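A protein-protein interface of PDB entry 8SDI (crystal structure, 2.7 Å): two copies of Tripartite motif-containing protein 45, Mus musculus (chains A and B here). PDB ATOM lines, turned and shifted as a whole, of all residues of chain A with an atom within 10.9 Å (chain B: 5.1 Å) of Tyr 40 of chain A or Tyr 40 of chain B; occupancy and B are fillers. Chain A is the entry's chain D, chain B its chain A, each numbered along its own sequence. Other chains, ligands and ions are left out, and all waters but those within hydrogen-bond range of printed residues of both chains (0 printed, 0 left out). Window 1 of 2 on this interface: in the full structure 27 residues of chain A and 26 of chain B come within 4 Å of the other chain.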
ATOM      1  N   ALA A  31     -24.896  -2.598   6.549  1.00  0.00           N
ATOM      2  CA  ALA A  31     -24.329  -2.044   5.329  1.00  0.00           C
ATOM      3  C   ALA A  31     -24.242  -0.521   5.431  1.00  0.00           C
ATOM      4  O   ALA A  31     -23.204   0.061   5.123  1.00  0.00           O
ATOM      5  CB  ALA A  31     -25.123  -2.460   4.110  1.00  0.00           C
ATOM      6  N   ASP A  32     -25.336   0.124   5.853  1.00  0.00           N
ATOM      7  CA  ASP A  32     -25.395   1.576   5.814  1.00  0.00           C
ATOM      8  C   ASP A  32     -24.428   2.155   6.842  1.00  0.00           C
ATOM      9  O   ASP A  32     -23.605   3.012   6.520  1.00  0.00           O
ATOM     10  CB  ASP A  32     -26.830   2.104   5.832  1.00  0.00           C
ATOM     11  CG  ASP A  32     -27.562   1.780   4.533  1.00  0.00           C
ATOM     12  OD1 ASP A  32     -26.943   1.165   3.624  1.00  0.00           O
ATOM     13  OD2 ASP A  32     -28.758   2.112   4.440  1.00  0.00           O
ATOM     14  N   VAL A  33     -24.480   1.635   8.062  1.00  0.00           N
ATOM     15  CA  VAL A  33     -23.517   2.047   9.061  1.00  0.00           C
ATOM     16  C   VAL A  33     -22.122   2.077   8.442  1.00  0.00           C
ATOM     17  O   VAL A  33     -21.365   3.005   8.720  1.00  0.00           O
ATOM     18  CB  VAL A  33     -23.620   1.133  10.291  1.00  0.00           C
ATOM     19  CG1 VAL A  33     -22.386   1.168  11.179  1.00  0.00           C
ATOM     20  CG2 VAL A  33     -24.891   1.406  11.088  1.00  0.00           C
ATOM     21  N   ARG A  34     -21.806   1.091   7.578  1.00  0.00           N
ATOM     22  CA  ARG A  34     -20.516   0.963   6.891  1.00  0.00           C
ATOM     23  C   ARG A  34     -20.210   2.148   5.967  1.00  0.00           C
ATOM     24  O   ARG A  34     -19.198   2.822   6.143  1.00  0.00           O
ATOM     25  CB  ARG A  34     -20.477  -0.293   6.022  1.00  0.00           C
ATOM     26  CG  ARG A  34     -20.280  -1.579   6.809  1.00  0.00           C
ATOM     27  CD  ARG A  34     -19.819  -2.765   5.987  1.00  0.00           C
ATOM     28  NE  ARG A  34     -19.364  -3.726   6.989  1.00  0.00           N
ATOM     29  CZ  ARG A  34     -20.133  -4.657   7.532  1.00  0.00           C
ATOM     30  NH1 ARG A  34     -21.394  -4.779   7.136  1.00  0.00           N
ATOM     31  NH2 ARG A  34     -19.627  -5.454   8.460  1.00  0.00           N
ATOM     32  N   THR A  35     -21.061   2.360   4.952  1.00  0.00           N
ATOM     33  CA  THR A  35     -20.957   3.492   4.040  1.00  0.00           C
ATOM     34  C   THR A  35     -20.904   4.829   4.781  1.00  0.00           C
ATOM     35  O   THR A  35     -20.064   5.654   4.445  1.00  0.00           O
ATOM     36  CB  THR A  35     -22.176   3.611   3.124  1.00  0.00           C
ATOM     37  OG1 THR A  35     -22.615   2.313   2.747  1.00  0.00           O
ATOM     38  CG2 THR A  35     -21.900   4.432   1.890  1.00  0.00           C
ATOM     39  N   PHE A  36     -21.827   5.080   5.728  1.00  0.00           N
ATOM     40  CA  PHE A  36     -21.743   6.317   6.489  1.00  0.00           C
ATOM     41  C   PHE A  36     -20.352   6.467   7.100  1.00  0.00           C
ATOM     42  O   PHE A  36     -19.702   7.490   6.874  1.00  0.00           O
ATOM     43  CB  PHE A  36     -22.842   6.490   7.539  1.00  0.00           C
ATOM     44  CG  PHE A  36     -24.231   6.214   7.026  1.00  0.00           C
ATOM     45  CD1 PHE A  36     -24.506   6.197   5.662  1.00  0.00           C
ATOM     46  CD2 PHE A  36     -25.284   5.995   7.919  1.00  0.00           C
ATOM     47  CE1 PHE A  36     -25.806   5.956   5.218  1.00  0.00           C
ATOM     48  CE2 PHE A  36     -26.580   5.754   7.475  1.00  0.00           C
ATOM     49  CZ  PHE A  36     -26.836   5.731   6.120  1.00  0.00           C
ATOM     50  N   SER A  37     -19.867   5.456   7.835  1.00  0.00           N
ATOM     51  CA  SER A  37     -18.639   5.735   8.571  1.00  0.00           C
ATOM     52  C   SER A  37     -17.500   6.002   7.602  1.00  0.00           C
ATOM     53  O   SER A  37     -16.650   6.855   7.863  1.00  0.00           O
ATOM     54  CB  SER A  37     -18.257   4.656   9.505  1.00  0.00           C
ATOM     55  OG  SER A  37     -19.389   4.182  10.206  1.00  0.00           O
ATOM     56  N   GLU A  38     -17.506   5.237   6.504  1.00  0.00           N
ATOM     57  CA  GLU A  38     -16.511   5.344   5.455  1.00  0.00           C
ATOM     58  C   GLU A  38     -16.620   6.719   4.810  1.00  0.00           C
ATOM     59  O   GLU A  38     -15.630   7.435   4.728  1.00  0.00           O
ATOM     60  CB  GLU A  38     -16.733   4.238   4.423  1.00  0.00           C
ATOM     61  CG  GLU A  38     -15.899   4.399   3.162  1.00  0.00           C
ATOM     62  CD  GLU A  38     -16.289   3.503   1.993  1.00  0.00           C
ATOM     63  OE1 GLU A  38     -15.378   2.887   1.388  1.00  0.00           O
ATOM     64  OE2 GLU A  38     -17.499   3.431   1.683  1.00  0.00           O
ATOM     65  N   GLY A  39     -17.822   7.053   4.327  1.00  0.00           N
ATOM     66  CA  GLY A  39     -18.156   8.375   3.809  1.00  0.00           C
ATOM     67  C   GLY A  39     -17.709   9.509   4.741  1.00  0.00           C
ATOM     68  O   GLY A  39     -17.165  10.502   4.259  1.00  0.00           O
ATOM     69  N   TYR A  40     -17.893   9.325   6.027  1.00  0.00           N
ATOM     70  CA  TYR A  40     -17.508  10.394   6.936  1.00  0.00           C
ATOM     71  C   TYR A  40     -16.001  10.519   6.907  1.00  0.00           C
ATOM     72  O   TYR A  40     -15.472  11.561   6.544  1.00  0.00           O
ATOM     73  CB  TYR A  40     -17.775  10.132   8.425  1.00  0.00           C
ATOM     74  CG  TYR A  40     -19.221  10.171   8.837  1.00  0.00           C
ATOM     75  CD1 TYR A  40     -20.019  11.271   8.555  1.00  0.00           C
ATOM     76  CD2 TYR A  40     -19.789   9.089   9.500  1.00  0.00           C
ATOM     77  CE1 TYR A  40     -21.357  11.287   8.929  1.00  0.00           C
ATOM     78  CE2 TYR A  40     -21.130   9.077   9.850  1.00  0.00           C
ATOM     79  CZ  TYR A  40     -21.911  10.185   9.569  1.00  0.00           C
ATOM     80  OH  TYR A  40     -23.222  10.141   9.918  1.00  0.00           O
ATOM     81  N   ILE A  41     -15.336   9.452   7.238  1.00  0.00           N
ATOM     82  CA  ILE A  41     -13.916   9.518   7.504  1.00  0.00           C
ATOM     83  C   ILE A  41     -13.226  10.199   6.331  1.00  0.00           C
ATOM     84  O   ILE A  41     -12.339  11.017   6.546  1.00  0.00           O
ATOM     85  CB  ILE A  41     -13.341   8.129   7.775  1.00  0.00           C
ATOM     86  CG1 ILE A  41     -13.976   7.553   9.041  1.00  0.00           C
ATOM     87  CG2 ILE A  41     -11.842   8.289   7.882  1.00  0.00           C
ATOM     88  CD1 ILE A  41     -13.633   6.130   9.362  1.00  0.00           C
ATOM     89  N   LYS A  42     -13.685   9.890   5.112  1.00  0.00           N
ATOM     90  CA  LYS A  42     -13.191  10.551   3.912  1.00  0.00           C
ATOM     91  C   LYS A  42     -13.317  12.060   4.082  1.00  0.00           C
ATOM     92  O   LYS A  42     -12.304  12.771   4.109  1.00  0.00           O
ATOM     93  CB  LYS A  42     -13.941  10.105   2.649  1.00  0.00           C
ATOM     94  CG  LYS A  42     -13.107  10.162   1.373  1.00  0.00           C
ATOM     95  CD  LYS A  42     -13.808   9.732   0.093  1.00  0.00           C
ATOM     96  CE  LYS A  42     -14.295   8.296   0.103  1.00  0.00           C
ATOM     97  NZ  LYS A  42     -13.206   7.337  -0.199  1.00  0.00           N
ATOM     98  N   ALA A  43     -14.577  12.517   4.185  1.00  0.00           N
ATOM     99  CA  ALA A  43     -14.910  13.926   4.362  1.00  0.00           C
ATOM    100  C   ALA A  43     -14.009  14.553   5.416  1.00  0.00           C
ATOM    101  O   ALA A  43     -13.495  15.632   5.174  1.00  0.00           O
ATOM    102  CB  ALA A  43     -16.360  14.131   4.707  1.00  0.00           C
ATOM    103  N   ILE A  44     -13.802  13.891   6.563  1.00  0.00           N
ATOM    104  CA  ILE A  44     -12.950  14.489   7.585  1.00  0.00           C
ATOM    105  C   ILE A  44     -11.543  14.661   7.032  1.00  0.00           C
ATOM    106  O   ILE A  44     -10.990  15.756   7.092  1.00  0.00           O
ATOM    107  CB  ILE A  44     -12.987  13.722   8.913  1.00  0.00           C
ATOM    108  CG1 ILE A  44     -14.416  13.697   9.448  1.00  0.00           C
ATOM    109  CG2 ILE A  44     -12.014  14.291   9.933  1.00  0.00           C
ATOM    110  CD1 ILE A  44     -14.668  12.513  10.334  1.00  0.00           C
ATOM    111  N   GLU A  45     -11.001  13.608   6.411  1.00  0.00           N
ATOM    112  CA  GLU A  45      -9.634  13.684   5.924  1.00  0.00           C
ATOM    113  C   GLU A  45      -9.526  14.845   4.940  1.00  0.00           C
ATOM    114  O   GLU A  45      -8.736  15.762   5.171  1.00  0.00           O
ATOM    115  CB  GLU A  45      -9.136  12.317   5.452  1.00  0.00           C
ATOM    116  CG  GLU A  45      -8.897  11.363   6.617  1.00  0.00           C
ATOM    117  CD  GLU A  45      -9.016   9.876   6.302  1.00  0.00           C
ATOM    118  OE1 GLU A  45      -9.618   9.546   5.251  1.00  0.00           O
ATOM    119  OE2 GLU A  45      -8.510   9.044   7.113  1.00  0.00           O
ATOM    120  N   GLU A  46     -10.405  14.848   3.926  1.00  0.00           N
ATOM    121  CA  GLU A  46     -10.436  15.885   2.896  1.00  0.00           C
ATOM    122  C   GLU A  46     -10.449  17.309   3.471  1.00  0.00           C
ATOM    123  O   GLU A  46      -9.673  18.165   3.043  1.00  0.00           O
ATOM    124  CB  GLU A  46     -11.599  15.675   1.928  1.00  0.00           C
ATOM    125  CG  GLU A  46     -11.451  14.404   1.119  1.00  0.00           C
ATOM    126  CD  GLU A  46     -12.631  14.116   0.208  1.00  0.00           C
ATOM    127  OE1 GLU A  46     -13.565  14.951   0.186  1.00  0.00           O
ATOM    128  OE2 GLU A  46     -12.608  13.061  -0.483  1.00  0.00           O
ATOM    129  N   HIS A  47     -11.337  17.577   4.433  1.00  0.00           N
ATOM    130  CA  HIS A  47     -11.447  18.907   5.003  1.00  0.00           C
ATOM    131  C   HIS A  47     -10.239  19.198   5.899  1.00  0.00           C
ATOM    132  O   HIS A  47      -9.711  20.316   5.895  1.00  0.00           O
ATOM    133  CB  HIS A  47     -12.798  19.077   5.717  1.00  0.00           C
ATOM    134  CG  HIS A  47     -14.022  18.865   4.873  1.00  0.00           C
ATOM    135  ND1 HIS A  47     -14.087  19.201   3.519  1.00  0.00           N
ATOM    136  CD2 HIS A  47     -15.256  18.405   5.201  1.00  0.00           C
ATOM    137  CE1 HIS A  47     -15.294  18.919   3.054  1.00  0.00           C
ATOM    138  NE2 HIS A  47     -16.032  18.426   4.066  1.00  0.00           N
ATOM    139  N   ARG A  48      -9.780  18.186   6.652  1.00  0.00           N
ATOM    140  CA  ARG A  48      -8.608  18.377   7.493  1.00  0.00           C
ATOM    141  C   ARG A  48      -7.422  18.788   6.628  1.00  0.00           C
ATOM    142  O   ARG A  48      -6.538  19.528   7.060  1.00  0.00           O
ATOM    143  CB  ARG A  48      -8.278  17.085   8.245  1.00  0.00           C
ATOM    144  CG  ARG A  48      -6.972  17.114   9.024  1.00  0.00           C
ATOM    145  CD  ARG A  48      -5.873  16.381   8.286  1.00  0.00           C
ATOM    146  NE  ARG A  48      -5.864  14.981   8.676  1.00  0.00           N
ATOM    147  CZ  ARG A  48      -6.234  13.968   7.899  1.00  0.00           C
ATOM    148  NH1 ARG A  48      -6.183  12.737   8.381  1.00  0.00           N
ATOM    149  NH2 ARG A  48      -6.645  14.182   6.654  1.00  0.00           N
ATOM    150  N   ASP A  49      -7.416  18.276   5.394  1.00  0.00           N
ATOM    151  CA  ASP A  49      -6.315  18.520   4.484  1.00  0.00           C
ATOM    152  C   ASP A  49      -6.378  19.897   3.855  1.00  0.00           C
ATOM    153  O   ASP A  49      -5.396  20.635   3.946  1.00  0.00           O
ATOM    154  CB  ASP A  49      -6.316  17.534   3.325  1.00  0.00           C
ATOM    155  CG  ASP A  49      -5.734  16.176   3.676  1.00  0.00           C
ATOM    156  OD1 ASP A  49      -5.101  16.035   4.792  1.00  0.00           O
ATOM    157  OD2 ASP A  49      -5.924  15.261   2.827  1.00  0.00           O
ATOM    158  N   LEU A  51      -7.845  22.362   5.002  1.00  0.00           N
ATOM    159  CA  LEU A  51      -7.578  23.362   6.015  1.00  0.00           C
ATOM    160  C   LEU A  51      -6.078  23.417   6.225  1.00  0.00           C
ATOM    161  O   LEU A  51      -5.470  24.461   6.037  1.00  0.00           O
ATOM    162  CB  LEU A  51      -8.328  23.075   7.325  1.00  0.00           C
ATOM    163  CG  LEU A  51      -9.859  23.240   7.315  1.00  0.00           C
ATOM    164  CD1 LEU A  51     -10.424  23.047   8.711  1.00  0.00           C
ATOM    165  CD2 LEU A  51     -10.334  24.569   6.725  1.00  0.00           C
ATOM    166  N   THR B  35     -19.015  26.222   6.238  1.00  0.00           N
ATOM    167  CA  THR B  35     -19.434  25.226   5.261  1.00  0.00           C
ATOM    168  C   THR B  35     -19.208  23.797   5.762  1.00  0.00           C
ATOM    169  O   THR B  35     -20.184  23.067   5.898  1.00  0.00           O
ATOM    170  CB  THR B  35     -18.751  25.444   3.905  1.00  0.00           C
ATOM    171  OG1 THR B  35     -19.112  26.748   3.460  1.00  0.00           O
ATOM    172  CG2 THR B  35     -19.190  24.451   2.853  1.00  0.00           C
ATOM    173  N   PHE B  36     -17.950  23.374   5.993  1.00  0.00           N
ATOM    174  CA  PHE B  36     -17.749  22.001   6.443  1.00  0.00           C
ATOM    175  C   PHE B  36     -18.624  21.720   7.657  1.00  0.00           C
ATOM    176  O   PHE B  36     -19.307  20.701   7.687  1.00  0.00           O
ATOM    177  CB  PHE B  36     -16.298  21.641   6.769  1.00  0.00           C
ATOM    178  CG  PHE B  36     -15.298  22.069   5.725  1.00  0.00           C
ATOM    179  CD1 PHE B  36     -15.679  22.226   4.388  1.00  0.00           C
ATOM    180  CD2 PHE B  36     -13.961  22.287   6.071  1.00  0.00           C
ATOM    181  CE1 PHE B  36     -14.739  22.600   3.430  1.00  0.00           C
ATOM    182  CE2 PHE B  36     -13.024  22.667   5.115  1.00  0.00           C
ATOM    183  CZ  PHE B  36     -13.420  22.825   3.794  1.00  0.00           C
ATOM    184  N   SER B  37     -18.627  22.633   8.637  1.00  0.00           N
ATOM    185  CA  SER B  37     -19.285  22.320   9.896  1.00  0.00           C
ATOM    186  C   SER B  37     -20.789  22.199   9.720  1.00  0.00           C
ATOM    187  O   SER B  37     -21.429  21.390  10.387  1.00  0.00           O
ATOM    188  CB  SER B  37     -18.953  23.306  10.940  1.00  0.00           C
ATOM    189  OG  SER B  37     -17.792  22.887  11.632  1.00  0.00           O
ATOM    190  N   GLU B  38     -21.340  23.012   8.817  1.00  0.00           N
ATOM    191  CA  GLU B  38     -22.764  22.989   8.563  1.00  0.00           C
ATOM    192  C   GLU B  38     -23.112  21.712   7.807  1.00  0.00           C
ATOM    193  O   GLU B  38     -23.967  20.957   8.268  1.00  0.00           O
ATOM    194  CB  GLU B  38     -23.152  24.221   7.752  1.00  0.00           C
ATOM    195  CG  GLU B  38     -24.521  24.787   8.084  1.00  0.00           C
ATOM    196  CD  GLU B  38     -24.801  26.088   7.342  1.00  0.00           C
ATOM    197  OE1 GLU B  38     -23.821  26.701   6.844  1.00  0.00           O
ATOM    198  OE2 GLU B  38     -25.994  26.490   7.259  1.00  0.00           O
ATOM    199  N   GLY B  39     -22.489  21.526   6.627  1.00  0.00           N
ATOM    200  CA  GLY B  39     -22.608  20.311   5.830  1.00  0.00           C
ATOM    201  C   GLY B  39     -22.400  19.049   6.681  1.00  0.00           C
ATOM    202  O   GLY B  39     -23.137  18.069   6.579  1.00  0.00           O
ATOM    203  N   TYR B  40     -21.424  19.083   7.586  1.00  0.00           N
ATOM    204  CA  TYR B  40     -21.206  17.919   8.418  1.00  0.00           C
ATOM    205  C   TYR B  40     -22.417  17.602   9.287  1.00  0.00           C
ATOM    206  O   TYR B  40     -22.906  16.479   9.243  1.00  0.00           O
ATOM    207  CB  TYR B  40     -19.945  18.049   9.270  1.00  0.00           C
ATOM    208  CG  TYR B  40     -19.281  16.717   9.465  1.00  0.00           C
ATOM    209  CD1 TYR B  40     -19.772  15.814  10.401  1.00  0.00           C
ATOM    210  CD2 TYR B  40     -18.215  16.329   8.669  1.00  0.00           C
ATOM    211  CE1 TYR B  40     -19.204  14.561  10.580  1.00  0.00           C
ATOM    212  CE2 TYR B  40     -17.631  15.080   8.842  1.00  0.00           C
ATOM    213  CZ  TYR B  40     -18.124  14.195   9.797  1.00  0.00           C
ATOM    214  OH  TYR B  40     -17.577  12.958   9.983  1.00  0.00           O
ATOM    215  N   ILE B  41     -22.840  18.551  10.128  1.00  0.00           N
ATOM    216  CA  ILE B  41     -23.932  18.312  11.059  1.00  0.00           C
ATOM    217  C   ILE B  41     -25.149  17.777  10.315  1.00  0.00           C
ATOM    218  O   ILE B  41     -25.827  16.872  10.793  1.00  0.00           O
ATOM    219  CB  ILE B  41     -24.339  19.600  11.778  1.00  0.00           C
ATOM    220  CG1 ILE B  41     -23.296  19.993  12.820  1.00  0.00           C
ATOM    221  CG2 ILE B  41     -25.699  19.364  12.401  1.00  0.00           C
ATOM    222  CD1 ILE B  41     -23.405  21.407  13.312  1.00  0.00           C
ATOM    223  N   LYS B  42     -25.436  18.396   9.171  1.00  0.00           N
ATOM    224  CA  LYS B  42     -26.546  17.985   8.326  1.00  0.00           C
ATOM    225  C   LYS B  42     -26.471  16.484   8.033  1.00  0.00           C
ATOM    226  O   LYS B  42     -27.355  15.735   8.468  1.00  0.00           O
ATOM    227  CB  LYS B  42     -26.585  18.823   7.041  1.00  0.00           C
ATOM    228  CG  LYS B  42     -27.832  18.663   6.184  1.00  0.00           C
ATOM    229  CD  LYS B  42     -27.646  19.234   4.798  1.00  0.00           C
ATOM    230  CE  LYS B  42     -28.888  19.888   4.228  1.00  0.00           C
ATOM    231  NZ  LYS B  42     -29.753  18.911   3.519  1.00  0.00           N
ATOM    232  N   ALA B  43     -25.428  16.077   7.277  1.00  0.00           N
ATOM    233  CA  ALA B  43     -25.158  14.684   6.925  1.00  0.00           C
ATOM    234  C   ALA B  43     -25.346  13.768   8.126  1.00  0.00           C
ATOM    235  O   ALA B  43     -25.967  12.721   7.979  1.00  0.00           O
ATOM    236  CB  ALA B  43     -23.777  14.502   6.364  1.00  0.00           C
ATOM    237  N   ILE B  44     -24.834  14.161   9.305  1.00  0.00           N
ATOM    238  CA  ILE B  44     -25.137  13.415  10.525  1.00  0.00           C
ATOM    239  C   ILE B  44     -26.644  13.248  10.702  1.00  0.00           C
ATOM    240  O   ILE B  44     -27.129  12.121  10.723  1.00  0.00           O
ATOM    241  CB  ILE B  44     -24.446  13.950  11.792  1.00  0.00           C
ATOM    242  CG1 ILE B  44     -22.943  13.674  11.767  1.00  0.00           C
ATOM    243  CG2 ILE B  44     -25.072  13.331  13.025  1.00  0.00           C
ATOM    244  CD1 ILE B  44     -22.128  14.850  12.197  1.00  0.00           C
ATOM    245  N   HIS B  47     -28.226  10.807   8.151  1.00  0.00           N
ATOM    246  CA  HIS B  47     -27.812   9.432   8.399  1.00  0.00           C
ATOM    247  C   HIS B  47     -28.442   8.903   9.686  1.00  0.00           C
ATOM    248  O   HIS B  47     -28.886   7.752   9.729  1.00  0.00           O
ATOM    249  CB  HIS B  47     -26.281   9.308   8.424  1.00  0.00           C
ATOM    250  CG  HIS B  47     -25.574   9.626   7.137  1.00  0.00           C
ATOM    251  ND1 HIS B  47     -26.201   9.602   5.890  1.00  0.00           N
ATOM    252  CD2 HIS B  47     -24.274   9.928   6.892  1.00  0.00           C
ATOM    253  CE1 HIS B  47     -25.324   9.911   4.948  1.00  0.00           C
ATOM    254  NE2 HIS B  47     -24.135  10.117   5.537  1.00  0.00           N
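Among the printed residues, merely in contact across the chains: Ile 44 of chain A with Tyr 40 of chain B (3.0 Å), Tyr 40 of chain A with His 47 of chain B (3.2 Å), Tyr 40 of chain A with Tyr 40 of chain B (3.2 Å), His 47 of chain A with Phe 36 of chain B (3.4 Å), Phe 36 of chain A with His 47 of chain B (3.5 Å), Leu 51 of chain A with Phe 36 of chain B (3.7 Å) and Tyr 40 of chain A with Ile 44 of chain B (3.8 Å).
Printed residues of chain B within 4 Å of Tyr 40 of chain A: Tyr 40, Ile 44 and His 47. Of the printed residues of chain B, His 47 of chain A touches Phe 36. Printed residues of chain B within 4 Å of Leu 51 of chain A: Phe 36 (3.7 Å). No residue of chain A comes within 4 Å of Ser 37 of chain B. No residue of chain A comes within 4 Å of Gly 39 of chain B. Tyr 40 of chain B touches two residues of chain A. No residue of chain A comes within 4 Å of Ile 41 of chain B. The nearest printed residue of chain B that does not touch Phe 36 of chain A is Tyr 40 of chain B (6.6 Å).
Printed residues of chain B that touch a printed residue of chain A: Phe 36, Tyr 40, Ile 44 and His 47. Hydrophobic or aromatic side chains of chain A that line the printed part of chain B: Phe 36, Tyr 40, Ile 44, His 47 and Leu 51. Among the printed residues, 7 pairs touch across the chains. Among the printed residues, no Asp or Glu carboxylate lies within 4 Å of a Lys or Arg side-chain nitrogen of the other chain.
Phe 36 of chain A touches His 47 of chain B, and with the chains exchanged His 47 of chain A touches Phe 36 of chain B. Tyr 40 of chain A touches its own counterpart, Tyr 40 of chain B. Tyr 40 of chain A touches Ile 44 of chain B, and with the chains exchanged Ile 44 of chain A touches Tyr 40 of chain B. Tyr 40 of chain A touches His 47 of chain B, but with the chains exchanged His 47 of chain A does not touch Tyr 40 of chain B (5.0 Å).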
